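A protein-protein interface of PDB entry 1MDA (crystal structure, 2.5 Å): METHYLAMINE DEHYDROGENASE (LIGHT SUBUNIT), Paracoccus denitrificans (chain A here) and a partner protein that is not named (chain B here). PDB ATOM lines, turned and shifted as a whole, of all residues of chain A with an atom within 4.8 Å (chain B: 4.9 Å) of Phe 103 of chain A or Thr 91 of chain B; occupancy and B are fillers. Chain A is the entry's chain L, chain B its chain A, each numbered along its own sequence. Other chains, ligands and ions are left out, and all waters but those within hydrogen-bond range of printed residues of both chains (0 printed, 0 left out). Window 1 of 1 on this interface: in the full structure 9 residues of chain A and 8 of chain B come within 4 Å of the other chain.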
ATOM      1  N   ALA A  47       2.330 -14.418  17.166  1.00  0.00           N
ATOM      2  CA  ALA A  47       1.994 -13.443  18.182  1.00  0.00           C
ATOM      3  C   ALA A  47       0.560 -13.593  18.617  1.00  0.00           C
ATOM      4  O   ALA A  47      -0.176 -14.359  18.007  1.00  0.00           O
ATOM      5  CB  ALA A  47       2.144 -12.044  17.619  1.00  0.00           C
ATOM      6  N   SER A  48       0.240 -12.868  19.697  1.00  0.00           N
ATOM      7  CA  SER A  48      -1.079 -12.669  20.267  1.00  0.00           C
ATOM      8  C   SER A  48      -1.599 -11.316  19.831  1.00  0.00           C
ATOM      9  O   SER A  48      -2.754 -11.141  19.446  1.00  0.00           O
ATOM     10  CB  SER A  48      -1.134 -12.768  21.793  1.00  0.00           C
ATOM     11  OG  SER A  48      -1.469 -14.100  22.142  1.00  0.00           O
ATOM     12  N   GLY A  49      -0.691 -10.356  19.901  1.00  0.00           N
ATOM     13  CA  GLY A  49      -1.000  -9.022  19.472  1.00  0.00           C
ATOM     14  C   GLY A  49      -1.343  -9.005  17.986  1.00  0.00           C
ATOM     15  O   GLY A  49      -0.926  -9.840  17.172  1.00  0.00           O
ATOM     16  N   ILE A 100       5.214  -3.190  15.260  1.00  0.00           N
ATOM     17  CA  ILE A 100       5.444  -4.601  15.080  1.00  0.00           C
ATOM     18  C   ILE A 100       4.691  -5.388  16.155  1.00  0.00           C
ATOM     19  O   ILE A 100       5.008  -5.438  17.339  1.00  0.00           O
ATOM     20  CB  ILE A 100       6.915  -4.941  14.890  1.00  0.00           C
ATOM     21  CG1 ILE A 100       7.622  -5.337  16.150  1.00  0.00           C
ATOM     22  CG2 ILE A 100       7.682  -3.789  14.268  1.00  0.00           C
ATOM     23  CD1 ILE A 100       7.678  -6.850  16.214  1.00  0.00           C
ATOM     24  N   TRP A 101       3.576  -5.907  15.721  1.00  0.00           N
ATOM     25  CA  TRP A 101       2.701  -6.678  16.545  1.00  0.00           C
ATOM     26  C   TRP A 101       3.284  -8.068  16.727  1.00  0.00           C
ATOM     27  O   TRP A 101       2.952  -8.975  15.971  1.00  0.00           O
ATOM     28  CB  TRP A 101       1.336  -6.729  15.807  1.00  0.00           C
ATOM     29  CG  TRP A 101       0.651  -5.388  15.769  1.00  0.00           C
ATOM     30  CD1 TRP A 101      -0.008  -4.758  14.772  1.00  0.00           C
ATOM     31  CD2 TRP A 101       0.236  -4.667  16.916  1.00  0.00           C
ATOM     32  NE1 TRP A 101      -0.561  -3.620  15.149  1.00  0.00           N
ATOM     33  CE2 TRP A 101      -0.484  -3.555  16.481  1.00  0.00           C
ATOM     34  CE3 TRP A 101       0.442  -4.824  18.261  1.00  0.00           C
ATOM     35  CZ2 TRP A 101      -1.023  -2.627  17.333  1.00  0.00           C
ATOM     36  CZ3 TRP A 101      -0.052  -3.880  19.114  1.00  0.00           C
ATOM     37  CH2 TRP A 101      -0.723  -2.774  18.650  1.00  0.00           C
ATOM     38  N   CYS A 102       4.067  -8.297  17.777  1.00  0.00           N
ATOM     39  CA  CYS A 102       4.657  -9.629  18.031  1.00  0.00           C
ATOM     40  C   CYS A 102       4.454 -10.103  19.461  1.00  0.00           C
ATOM     41  O   CYS A 102       5.143 -11.014  19.890  1.00  0.00           O
ATOM     42  CB  CYS A 102       6.191  -9.738  17.775  1.00  0.00           C
ATOM     43  SG  CYS A 102       6.583 -10.180  16.082  1.00  0.00           S
ATOM     44  N   PHE A 103       3.571  -9.481  20.231  1.00  0.00           N
ATOM     45  CA  PHE A 103       3.422  -9.886  21.629  1.00  0.00           C
ATOM     46  C   PHE A 103       2.834 -11.294  21.863  1.00  0.00           C
ATOM     47  O   PHE A 103       1.620 -11.502  21.858  1.00  0.00           O
ATOM     48  CB  PHE A 103       2.811  -8.748  22.476  1.00  0.00           C
ATOM     49  CG  PHE A 103       3.370  -7.336  22.171  1.00  0.00           C
ATOM     50  CD1 PHE A 103       4.530  -6.864  22.788  1.00  0.00           C
ATOM     51  CD2 PHE A 103       2.744  -6.479  21.263  1.00  0.00           C
ATOM     52  CE1 PHE A 103       5.060  -5.601  22.508  1.00  0.00           C
ATOM     53  CE2 PHE A 103       3.222  -5.192  20.999  1.00  0.00           C
ATOM     54  CZ  PHE A 103       4.384  -4.746  21.635  1.00  0.00           C
ATOM     55  N   GLY A 104       3.740 -12.266  22.044  1.00  0.00           N
ATOM     56  CA  GLY A 104       3.495 -13.694  22.283  1.00  0.00           C
ATOM     57  C   GLY A 104       4.506 -14.542  21.448  1.00  0.00           C
ATOM     58  O   GLY A 104       4.658 -14.303  20.236  1.00  0.00           O
ATOM     59  N   MET A 109      10.117 -10.697  19.105  1.00  0.00           N
ATOM     60  CA  MET A 109       9.804  -9.323  18.777  1.00  0.00           C
ATOM     61  C   MET A 109      10.251  -8.992  17.358  1.00  0.00           C
ATOM     62  O   MET A 109      10.168  -7.858  16.904  1.00  0.00           O
ATOM     63  CB  MET A 109      10.402  -8.335  19.784  1.00  0.00           C
ATOM     64  CG  MET A 109       9.662  -8.324  21.098  1.00  0.00           C
ATOM     65  SD  MET A 109       7.905  -8.032  20.816  1.00  0.00           S
ATOM     66  CE  MET A 109       7.832  -6.375  20.099  1.00  0.00           C
ATOM     67  N   ASN B  52      -7.609  -9.802  25.230  1.00  0.00           N
ATOM     68  CA  ASN B  52      -7.186 -10.786  26.176  1.00  0.00           C
ATOM     69  C   ASN B  52      -7.045 -10.110  27.492  1.00  0.00           C
ATOM     70  O   ASN B  52      -7.041  -8.887  27.586  1.00  0.00           O
ATOM     71  CB  ASN B  52      -5.796 -11.405  25.833  1.00  0.00           C
ATOM     72  CG  ASN B  52      -4.612 -10.481  26.026  1.00  0.00           C
ATOM     73  OD1 ASN B  52      -4.350  -9.581  25.226  1.00  0.00           O
ATOM     74  ND2 ASN B  52      -3.968 -10.652  27.176  1.00  0.00           N
ATOM     75  N   HIS B  54      -4.216 -10.103  30.194  1.00  0.00           N
ATOM     76  CA  HIS B  54      -2.876 -10.357  30.630  1.00  0.00           C
ATOM     77  C   HIS B  54      -2.477  -9.488  31.785  1.00  0.00           C
ATOM     78  O   HIS B  54      -2.538  -8.276  31.691  1.00  0.00           O
ATOM     79  CB  HIS B  54      -1.904 -10.355  29.454  1.00  0.00           C
ATOM     80  CG  HIS B  54      -0.474 -10.083  29.778  1.00  0.00           C
ATOM     81  ND1 HIS B  54       0.244  -9.197  28.993  1.00  0.00           N
ATOM     82  CD2 HIS B  54       0.317 -10.480  30.811  1.00  0.00           C
ATOM     83  CE1 HIS B  54       1.461  -9.148  29.480  1.00  0.00           C
ATOM     84  NE2 HIS B  54       1.537  -9.888  30.590  1.00  0.00           N
ATOM     85  N   HIS B  89      -4.113  -6.152  32.003  1.00  0.00           N
ATOM     86  CA  HIS B  89      -4.234  -5.304  30.831  1.00  0.00           C
ATOM     87  C   HIS B  89      -4.465  -6.138  29.622  1.00  0.00           C
ATOM     88  O   HIS B  89      -4.401  -7.361  29.721  1.00  0.00           O
ATOM     89  CB  HIS B  89      -2.950  -4.491  30.578  1.00  0.00           C
ATOM     90  CG  HIS B  89      -1.733  -5.282  30.201  1.00  0.00           C
ATOM     91  ND1 HIS B  89      -1.299  -5.378  28.881  1.00  0.00           N
ATOM     92  CD2 HIS B  89      -0.844  -5.969  30.967  1.00  0.00           C
ATOM     93  CE1 HIS B  89      -0.183  -6.122  28.883  1.00  0.00           C
ATOM     94  NE2 HIS B  89       0.110  -6.505  30.112  1.00  0.00           N
ATOM     95  N   CYS B  90      -4.901  -5.452  28.557  1.00  0.00           N
ATOM     96  CA  CYS B  90      -5.144  -6.066  27.253  1.00  0.00           C
ATOM     97  C   CYS B  90      -3.889  -5.882  26.452  1.00  0.00           C
ATOM     98  O   CYS B  90      -3.490  -4.763  26.151  1.00  0.00           O
ATOM     99  CB  CYS B  90      -6.362  -5.499  26.525  1.00  0.00           C
ATOM    100  SG  CYS B  90      -6.498  -6.080  24.824  1.00  0.00           S
ATOM    101  N   THR B  91      -3.239  -6.968  26.092  1.00  0.00           N
ATOM    102  CA  THR B  91      -2.010  -6.805  25.344  1.00  0.00           C
ATOM    103  C   THR B  91      -1.963  -5.953  24.070  1.00  0.00           C
ATOM    104  O   THR B  91      -1.211  -5.005  23.997  1.00  0.00           O
ATOM    105  CB  THR B  91      -0.969  -7.928  25.417  1.00  0.00           C
ATOM    106  OG1 THR B  91      -0.056  -7.760  24.364  1.00  0.00           O
ATOM    107  CG2 THR B  91      -1.549  -9.315  25.400  1.00  0.00           C
ATOM    108  N   PRO B  92      -2.757  -6.273  23.056  1.00  0.00           N
ATOM    109  CA  PRO B  92      -2.729  -5.544  21.792  1.00  0.00           C
ATOM    110  C   PRO B  92      -2.879  -4.024  21.912  1.00  0.00           C
ATOM    111  O   PRO B  92      -2.742  -3.245  20.954  1.00  0.00           O
ATOM    112  CB  PRO B  92      -3.878  -6.128  20.961  1.00  0.00           C
ATOM    113  CG  PRO B  92      -4.687  -7.054  21.855  1.00  0.00           C
ATOM    114  CD  PRO B  92      -3.905  -7.213  23.145  1.00  0.00           C
ATOM    115  N   HIS B  93      -3.183  -3.605  23.126  1.00  0.00           N
ATOM    116  CA  HIS B  93      -3.403  -2.225  23.439  1.00  0.00           C
ATOM    117  C   HIS B  93      -3.241  -2.257  24.939  1.00  0.00           C
ATOM    118  O   HIS B  93      -4.211  -2.424  25.663  1.00  0.00           O
ATOM    119  CB  HIS B  93      -4.874  -1.870  23.151  1.00  0.00           C
ATOM    120  CG  HIS B  93      -5.612  -2.900  22.333  1.00  0.00           C
ATOM    121  ND1 HIS B  93      -6.386  -3.832  22.986  1.00  0.00           N
ATOM    122  CD2 HIS B  93      -5.648  -3.195  20.999  1.00  0.00           C
ATOM    123  CE1 HIS B  93      -6.905  -4.640  22.077  1.00  0.00           C
ATOM    124  NE2 HIS B  93      -6.482  -4.284  20.875  1.00  0.00           N
ATOM    125  N   PRO B  94      -2.000  -2.119  25.410  1.00  0.00           N
ATOM    126  CA  PRO B  94      -1.693  -2.181  26.826  1.00  0.00           C
ATOM    127  C   PRO B  94      -2.491  -1.162  27.614  1.00  0.00           C
ATOM    128  O   PRO B  94      -2.353  -1.007  28.828  1.00  0.00           O
ATOM    129  CB  PRO B  94      -0.245  -1.709  26.926  1.00  0.00           C
ATOM    130  CG  PRO B  94      -0.070  -0.763  25.756  1.00  0.00           C
ATOM    131  CD  PRO B  94      -1.029  -1.243  24.695  1.00  0.00           C
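The backbone NH (N) of Thr 91 of chain B sits close to the side-chain amide oxygen (OD1) of Asn 52 of chain B (3.0 Å).
The backbone NH of Ser 48 of chain A lies within hydrogen-bond range of the backbone carbonyl oxygen of Phe 103 of chain A, at 2.9 Å.
The backbone NH of Gly 49 of chain A is in hydrogen-bond range of the backbone carbonyl oxygen of Phe 103 of chain A, at 3.2 Å.
Of the 9 printed residues of chain A, 2 touch a printed residue of chain B.
Hydrophobic or aromatic side chains of chain A within 4 Å of the printed part of chain B: Trp 101 and Phe 103.
Among the printed residues, no Asp or Glu carboxylate lies within 4 Å of a Lys or Arg side-chain nitrogen of the other chain.
Thr 91 of chain B touches just one residue of chain A: Phe 103.
Printed residues of chain A within 4 Å of Pro 92 of chain B: Trp 101 (3.1 Å).
Of the printed residues of chain B, Trp 101 of chain A touches Pro 92 (3.1 Å).
Asn 52 of chain B touches none of the printed residues of chain A.
Cys 102 of chain A touches none of the printed residues of chain B.
The nearest printed residue of chain B that does not touch Trp 101 of chain A is His 93 of chain B (5.1 Å).
Among the printed residues, pairs that only touch across the chains: Trp 101 of chain A with Pro 92 of chain B and Phe 103 of chain A with Thr 91 of chain B.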
